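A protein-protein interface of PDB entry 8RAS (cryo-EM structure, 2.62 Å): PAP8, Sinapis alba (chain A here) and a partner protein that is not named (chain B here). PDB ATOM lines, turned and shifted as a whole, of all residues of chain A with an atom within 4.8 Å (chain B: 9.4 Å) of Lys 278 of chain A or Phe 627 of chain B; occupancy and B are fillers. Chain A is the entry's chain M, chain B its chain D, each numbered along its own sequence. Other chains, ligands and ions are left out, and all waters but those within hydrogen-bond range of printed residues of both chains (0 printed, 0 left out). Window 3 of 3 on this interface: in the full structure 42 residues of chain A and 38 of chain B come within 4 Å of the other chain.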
ATOM      1  N   PHE A 243     -13.333 -15.746  -8.863  1.00  0.00           N
ATOM      2  CA  PHE A 243     -14.555 -15.907  -9.640  1.00  0.00           C
ATOM      3  C   PHE A 243     -15.683 -16.450  -8.771  1.00  0.00           C
ATOM      4  O   PHE A 243     -15.530 -17.474  -8.100  1.00  0.00           O
ATOM      5  CB  PHE A 243     -14.314 -16.843 -10.822  1.00  0.00           C
ATOM      6  CG  PHE A 243     -15.572 -17.447 -11.379  1.00  0.00           C
ATOM      7  CD1 PHE A 243     -16.475 -16.672 -12.086  1.00  0.00           C
ATOM      8  CD2 PHE A 243     -15.854 -18.789 -11.192  1.00  0.00           C
ATOM      9  CE1 PHE A 243     -17.632 -17.224 -12.597  1.00  0.00           C
ATOM     10  CE2 PHE A 243     -17.013 -19.346 -11.700  1.00  0.00           C
ATOM     11  CZ  PHE A 243     -17.902 -18.563 -12.404  1.00  0.00           C
ATOM     12  N   VAL A 244     -16.821 -15.756  -8.791  1.00  0.00           N
ATOM     13  CA  VAL A 244     -18.047 -16.227  -8.163  1.00  0.00           C
ATOM     14  C   VAL A 244     -19.206 -15.939  -9.108  1.00  0.00           C
ATOM     15  O   VAL A 244     -19.122 -15.078  -9.985  1.00  0.00           O
ATOM     16  CB  VAL A 244     -18.301 -15.577  -6.785  1.00  0.00           C
ATOM     17  CG1 VAL A 244     -17.431 -16.228  -5.725  1.00  0.00           C
ATOM     18  CG2 VAL A 244     -18.037 -14.086  -6.848  1.00  0.00           C
ATOM     19  N   ASP A 276     -21.103 -11.553   1.035  1.00  0.00           N
ATOM     20  CA  ASP A 276     -20.094 -12.466   0.507  1.00  0.00           C
ATOM     21  C   ASP A 276     -20.779 -13.471  -0.411  1.00  0.00           C
ATOM     22  O   ASP A 276     -21.489 -14.367   0.057  1.00  0.00           O
ATOM     23  CB  ASP A 276     -19.357 -13.169   1.642  1.00  0.00           C
ATOM     24  CG  ASP A 276     -18.086 -13.853   1.175  1.00  0.00           C
ATOM     25  OD1 ASP A 276     -17.688 -13.639   0.011  1.00  0.00           O
ATOM     26  OD2 ASP A 276     -17.484 -14.603   1.971  1.00  0.00           O
ATOM     27  N   ARG A 277     -20.567 -13.323  -1.720  1.00  0.00           N
ATOM     28  CA  ARG A 277     -21.178 -14.221  -2.691  1.00  0.00           C
ATOM     29  C   ARG A 277     -20.602 -15.628  -2.641  1.00  0.00           C
ATOM     30  O   ARG A 277     -21.166 -16.530  -3.268  1.00  0.00           O
ATOM     31  CB  ARG A 277     -21.026 -13.649  -4.102  1.00  0.00           C
ATOM     32  CG  ARG A 277     -21.527 -12.223  -4.248  1.00  0.00           C
ATOM     33  CD  ARG A 277     -22.951 -12.191  -4.776  1.00  0.00           C
ATOM     34  NE  ARG A 277     -23.478 -10.833  -4.839  1.00  0.00           N
ATOM     35  CZ  ARG A 277     -24.578 -10.486  -5.493  1.00  0.00           C
ATOM     36  NH1 ARG A 277     -25.297 -11.375  -6.158  1.00  0.00           N
ATOM     37  NH2 ARG A 277     -24.966  -9.214  -5.482  1.00  0.00           N
ATOM     38  N   LYS A 278     -19.499 -15.838  -1.922  1.00  0.00           N
ATOM     39  CA  LYS A 278     -18.895 -17.161  -1.823  1.00  0.00           C
ATOM     40  C   LYS A 278     -19.705 -18.127  -0.969  1.00  0.00           C
ATOM     41  O   LYS A 278     -19.429 -19.330  -1.004  1.00  0.00           O
ATOM     42  CB  LYS A 278     -17.481 -17.045  -1.251  1.00  0.00           C
ATOM     43  CG  LYS A 278     -16.428 -16.615  -2.256  1.00  0.00           C
ATOM     44  CD  LYS A 278     -15.037 -16.596  -1.637  1.00  0.00           C
ATOM     45  CE  LYS A 278     -14.384 -17.973  -1.664  1.00  0.00           C
ATOM     46  NZ  LYS A 278     -14.919 -18.889  -0.617  1.00  0.00           N
ATOM     47  N   ASP A 279     -20.687 -17.641  -0.209  1.00  0.00           N
ATOM     48  CA  ASP A 279     -21.380 -18.465   0.775  1.00  0.00           C
ATOM     49  C   ASP A 279     -22.854 -18.681   0.459  1.00  0.00           C
ATOM     50  O   ASP A 279     -23.573 -19.247   1.290  1.00  0.00           O
ATOM     51  CB  ASP A 279     -21.240 -17.845   2.168  1.00  0.00           C
ATOM     52  CG  ASP A 279     -19.798 -17.746   2.620  1.00  0.00           C
ATOM     53  OD1 ASP A 279     -19.015 -18.669   2.314  1.00  0.00           O
ATOM     54  OD2 ASP A 279     -19.448 -16.745   3.280  1.00  0.00           O
ATOM     55  N   ASP A 280     -23.328 -18.254  -0.706  1.00  0.00           N
ATOM     56  CA  ASP A 280     -24.736 -18.389  -1.046  1.00  0.00           C
ATOM     57  C   ASP A 280     -24.963 -19.608  -1.929  1.00  0.00           C
ATOM     58  O   ASP A 280     -24.063 -20.067  -2.637  1.00  0.00           O
ATOM     59  CB  ASP A 280     -25.262 -17.130  -1.741  1.00  0.00           C
ATOM     60  CG  ASP A 280     -24.329 -16.617  -2.818  1.00  0.00           C
ATOM     61  OD1 ASP A 280     -23.766 -17.438  -3.571  1.00  0.00           O
ATOM     62  OD2 ASP A 280     -24.165 -15.384  -2.917  1.00  0.00           O
ATOM     63  N   HIS B 623     -29.560 -27.520  -6.781  1.00  0.00           N
ATOM     64  CA  HIS B 623     -28.747 -26.816  -5.794  1.00  0.00           C
ATOM     65  C   HIS B 623     -27.530 -26.247  -6.514  1.00  0.00           C
ATOM     66  O   HIS B 623     -26.530 -26.940  -6.713  1.00  0.00           O
ATOM     67  CB  HIS B 623     -28.346 -27.744  -4.656  1.00  0.00           C
ATOM     68  CG  HIS B 623     -29.483 -28.129  -3.764  1.00  0.00           C
ATOM     69  ND1 HIS B 623     -29.405 -29.172  -2.866  1.00  0.00           N
ATOM     70  CD2 HIS B 623     -30.727 -27.612  -3.633  1.00  0.00           C
ATOM     71  CE1 HIS B 623     -30.551 -29.279  -2.220  1.00  0.00           C
ATOM     72  NE2 HIS B 623     -31.370 -28.345  -2.666  1.00  0.00           N
ATOM     73  N   TYR B 624     -27.618 -24.977  -6.894  1.00  0.00           N
ATOM     74  CA  TYR B 624     -26.579 -24.317  -7.671  1.00  0.00           C
ATOM     75  C   TYR B 624     -25.631 -23.586  -6.727  1.00  0.00           C
ATOM     76  O   TYR B 624     -26.064 -22.732  -5.944  1.00  0.00           O
ATOM     77  CB  TYR B 624     -27.210 -23.349  -8.670  1.00  0.00           C
ATOM     78  CG  TYR B 624     -26.409 -23.124  -9.931  1.00  0.00           C
ATOM     79  CD1 TYR B 624     -25.045 -23.377  -9.970  1.00  0.00           C
ATOM     80  CD2 TYR B 624     -27.021 -22.653 -11.084  1.00  0.00           C
ATOM     81  CE1 TYR B 624     -24.316 -23.168 -11.120  1.00  0.00           C
ATOM     82  CE2 TYR B 624     -26.299 -22.442 -12.239  1.00  0.00           C
ATOM     83  CZ  TYR B 624     -24.947 -22.700 -12.251  1.00  0.00           C
ATOM     84  OH  TYR B 624     -24.224 -22.492 -13.402  1.00  0.00           O
ATOM     85  N   GLU B 625     -24.349 -23.921  -6.798  1.00  0.00           N
ATOM     86  CA  GLU B 625     -23.336 -23.266  -5.985  1.00  0.00           C
ATOM     87  C   GLU B 625     -22.720 -22.099  -6.743  1.00  0.00           C
ATOM     88  O   GLU B 625     -22.646 -22.103  -7.975  1.00  0.00           O
ATOM     89  CB  GLU B 625     -22.238 -24.249  -5.579  1.00  0.00           C
ATOM     90  CG  GLU B 625     -22.731 -25.454  -4.805  1.00  0.00           C
ATOM     91  CD  GLU B 625     -21.654 -26.504  -4.628  1.00  0.00           C
ATOM     92  OE1 GLU B 625     -20.470 -26.183  -4.858  1.00  0.00           O
ATOM     93  OE2 GLU B 625     -21.992 -27.649  -4.263  1.00  0.00           O
ATOM     94  N   SER B 626     -22.274 -21.093  -5.991  1.00  0.00           N
ATOM     95  CA  SER B 626     -21.650 -19.922  -6.593  1.00  0.00           C
ATOM     96  C   SER B 626     -20.299 -20.233  -7.221  1.00  0.00           C
ATOM     97  O   SER B 626     -19.796 -19.416  -7.999  1.00  0.00           O
ATOM     98  CB  SER B 626     -21.496 -18.817  -5.551  1.00  0.00           C
ATOM     99  OG  SER B 626     -20.406 -19.081  -4.687  1.00  0.00           O
ATOM    100  N   PHE B 627     -19.703 -21.382  -6.906  1.00  0.00           N
ATOM    101  CA  PHE B 627     -18.433 -21.772  -7.499  1.00  0.00           C
ATOM    102  C   PHE B 627     -18.590 -22.409  -8.872  1.00  0.00           C
ATOM    103  O   PHE B 627     -17.582 -22.629  -9.550  1.00  0.00           O
ATOM    104  CB  PHE B 627     -17.696 -22.738  -6.568  1.00  0.00           C
ATOM    105  CG  PHE B 627     -16.803 -22.057  -5.571  1.00  0.00           C
ATOM    106  CD1 PHE B 627     -16.718 -20.676  -5.524  1.00  0.00           C
ATOM    107  CD2 PHE B 627     -16.049 -22.800  -4.678  1.00  0.00           C
ATOM    108  CE1 PHE B 627     -15.898 -20.049  -4.607  1.00  0.00           C
ATOM    109  CE2 PHE B 627     -15.227 -22.179  -3.759  1.00  0.00           C
ATOM    110  CZ  PHE B 627     -15.152 -20.800  -3.724  1.00  0.00           C
ATOM    111  N   GLY B 628     -19.819 -22.716  -9.295  1.00  0.00           N
ATOM    112  CA  GLY B 628     -20.092 -23.277 -10.608  1.00  0.00           C
ATOM    113  C   GLY B 628     -20.785 -24.625 -10.566  1.00  0.00           C
ATOM    114  O   GLY B 628     -21.615 -24.915 -11.434  1.00  0.00           O
ATOM    115  N   ASN B 629     -20.456 -25.455  -9.581  1.00  0.00           N
ATOM    116  CA  ASN B 629     -21.071 -26.771  -9.472  1.00  0.00           C
ATOM    117  C   ASN B 629     -22.539 -26.652  -9.088  1.00  0.00           C
ATOM    118  O   ASN B 629     -22.914 -25.825  -8.254  1.00  0.00           O
ATOM    119  CB  ASN B 629     -20.331 -27.618  -8.437  1.00  0.00           C
ATOM    120  CG  ASN B 629     -18.972 -28.076  -8.921  1.00  0.00           C
ATOM    121  OD1 ASN B 629     -18.002 -27.321  -8.885  1.00  0.00           O
ATOM    122  ND2 ASN B 629     -18.895 -29.322  -9.371  1.00  0.00           N
ATOM    123  N   TYR B 630     -23.377 -27.484  -9.702  1.00  0.00           N
ATOM    124  CA  TYR B 630     -24.778 -27.576  -9.323  1.00  0.00           C
ATOM    125  C   TYR B 630     -25.187 -29.038  -9.224  1.00  0.00           C
ATOM    126  O   TYR B 630     -24.692 -29.891  -9.964  1.00  0.00           O
ATOM    127  CB  TYR B 630     -25.707 -26.838 -10.308  1.00  0.00           C
ATOM    128  CG  TYR B 630     -25.435 -27.071 -11.779  1.00  0.00           C
ATOM    129  CD1 TYR B 630     -24.384 -26.436 -12.422  1.00  0.00           C
ATOM    130  CD2 TYR B 630     -26.252 -27.906 -12.527  1.00  0.00           C
ATOM    131  CE1 TYR B 630     -24.142 -26.641 -13.766  1.00  0.00           C
ATOM    132  CE2 TYR B 630     -26.018 -28.115 -13.871  1.00  0.00           C
ATOM    133  CZ  TYR B 630     -24.961 -27.480 -14.485  1.00  0.00           C
ATOM    134  OH  TYR B 630     -24.722 -27.684 -15.823  1.00  0.00           O
ATOM    135  N   ARG B 641     -23.121 -31.690 -11.811  1.00  0.00           N
ATOM    136  CA  ARG B 641     -22.541 -31.071 -12.990  1.00  0.00           C
ATOM    137  C   ARG B 641     -21.823 -29.791 -12.591  1.00  0.00           C
ATOM    138  O   ARG B 641     -22.053 -29.234 -11.515  1.00  0.00           O
ATOM    139  CB  ARG B 641     -23.603 -30.767 -14.052  1.00  0.00           C
ATOM    140  CG  ARG B 641     -24.236 -32.000 -14.665  1.00  0.00           C
ATOM    141  CD  ARG B 641     -24.832 -31.687 -16.023  1.00  0.00           C
ATOM    142  NE  ARG B 641     -26.203 -31.205 -15.913  1.00  0.00           N
ATOM    143  CZ  ARG B 641     -26.811 -30.467 -16.831  1.00  0.00           C
ATOM    144  NH1 ARG B 641     -26.199 -30.113 -17.949  1.00  0.00           N
ATOM    145  NH2 ARG B 641     -28.061 -30.071 -16.620  1.00  0.00           N
ATOM    146  N   SER B 642     -20.942 -29.332 -13.475  1.00  0.00           N
ATOM    147  CA  SER B 642     -20.177 -28.118 -13.246  1.00  0.00           C
ATOM    148  C   SER B 642     -20.097 -27.322 -14.539  1.00  0.00           C
ATOM    149  O   SER B 642     -20.198 -27.878 -15.636  1.00  0.00           O
ATOM    150  CB  SER B 642     -18.765 -28.427 -12.737  1.00  0.00           C
ATOM    151  OG  SER B 642     -18.042 -27.236 -12.487  1.00  0.00           O
ATOM    152  N   VAL B 643     -19.918 -26.009 -14.399  1.00  0.00           N
ATOM    153  CA  VAL B 643     -19.717 -25.155 -15.563  1.00  0.00           C
ATOM    154  C   VAL B 643     -18.242 -24.997 -15.915  1.00  0.00           C
ATOM    155  O   VAL B 643     -17.922 -24.640 -17.057  1.00  0.00           O
ATOM    156  CB  VAL B 643     -20.353 -23.770 -15.352  1.00  0.00           C
ATOM    157  CG1 VAL B 643     -21.840 -23.908 -15.075  1.00  0.00           C
ATOM    158  CG2 VAL B 643     -19.659 -23.031 -14.220  1.00  0.00           C
ATOM    159  N   LYS B 644     -17.336 -25.252 -14.969  1.00  0.00           N
ATOM    160  CA  LYS B 644     -15.910 -25.157 -15.255  1.00  0.00           C
ATOM    161  C   LYS B 644     -15.415 -26.370 -16.033  1.00  0.00           C
ATOM    162  O   LYS B 644     -14.723 -26.227 -17.047  1.00  0.00           O
ATOM    163  CB  LYS B 644     -15.121 -25.007 -13.954  1.00  0.00           C
ATOM    164  CG  LYS B 644     -15.481 -23.786 -13.130  1.00  0.00           C
ATOM    165  CD  LYS B 644     -14.231 -23.041 -12.696  1.00  0.00           C
ATOM    166  CE  LYS B 644     -14.221 -22.798 -11.198  1.00  0.00           C
ATOM    167  NZ  LYS B 644     -15.341 -21.922 -10.767  1.00  0.00           N
ATOM    168  N   LYS B 645     -15.761 -27.568 -15.575  1.00  0.00           N
ATOM    169  CA  LYS B 645     -15.273 -28.810 -16.153  1.00  0.00           C
ATOM    170  C   LYS B 645     -16.397 -29.528 -16.893  1.00  0.00           C
ATOM    171  O   LYS B 645     -17.555 -29.102 -16.893  1.00  0.00           O
ATOM    172  CB  LYS B 645     -14.679 -29.711 -15.067  1.00  0.00           C
ATOM    173  CG  LYS B 645     -14.230 -28.975 -13.818  1.00  0.00           C
ATOM    174  CD  LYS B 645     -13.782 -29.951 -12.741  1.00  0.00           C
ATOM    175  CE  LYS B 645     -14.188 -29.473 -11.357  1.00  0.00           C
ATOM    176  NZ  LYS B 645     -15.652 -29.619 -11.135  1.00  0.00           N
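The side-chain hydroxyl (OG) of Ser 626 of chain B is in hydrogen-bond range of the backbone carbonyl oxygen (O) of Arg 277 of chain A, 3.0 Å away.
O of Phe 627 of chain B sits at hydrogen-bond distance from NZ of Lys 644 of chain B, at 2.6 Å.
The side-chain carboxylate of Asp 276 of chain A lies close to the backbone NH of Lys 278 of chain A, at 3.4 Å.
The side-chain hydroxyl of Ser 642 of chain B sits at hydrogen-bond distance from the backbone NH of Lys 644 of chain B (3.3 Å).
Among the printed residues, merely in contact across the chains: Phe 243 of chain A with Phe 627 of chain B (3.97 Å), Phe 243 of chain A with Lys 644 of chain B (3.2 Å), Val 244 of chain A with Ser 626 of chain B (3.6 Å), Lys 278 of chain A with Ser 626 of chain B (3.8 Å), Lys 278 of chain A with Phe 627 of chain B (3.6 Å) and Asp 280 of chain A with Ser 626 of chain B (3.3 Å).
Lys 278 of chain A touches two residues of chain B.
Of chain A, only Phe 243 (3.97 Å) and Lys 278 (3.6 Å) come within 4 Å of Phe 627 of chain B.
No residue of chain B comes within 4 Å of Asp 279 of chain A.
Of the printed residues of chain B, Phe 243 of chain A touches Phe 627 and Lys 644.
Of the printed residues of chain A, Ser 626 of chain B touches Val 244 (3.6 Å), Arg 277 (3.0 Å), Lys 278 (3.8 Å) and Asp 280 (3.3 Å).
Printed residues of chain B within 4 Å of Asp 280 of chain A: Ser 626 (3.3 Å).
Lys 645 of chain B touches none of the printed residues of chain A.
The nearest residue of chain B that does not touch Lys 278 of chain A is Glu 625 of chain B (7.2 Å).
The nearest residue of chain A that does not touch Phe 627 of chain B is Val 244 of chain A (4.3 Å).
Of the 7 printed residues of chain A, 5 touch a printed residue of chain B.
Hydrophobic or aromatic side chains of chain A within 4 Å of the printed part of chain B: Phe 243.
Printed residues of chain B that touch a printed residue of chain A: Ser 626, Phe 627 and Lys 644.
Hydrophobic or aromatic side chains of chain B that line the printed part of chain A: Phe 627.
Among the printed residues, no Asp or Glu carboxylate lies within 4 Å of a Lys or Arg side-chain nitrogen of the other chain.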
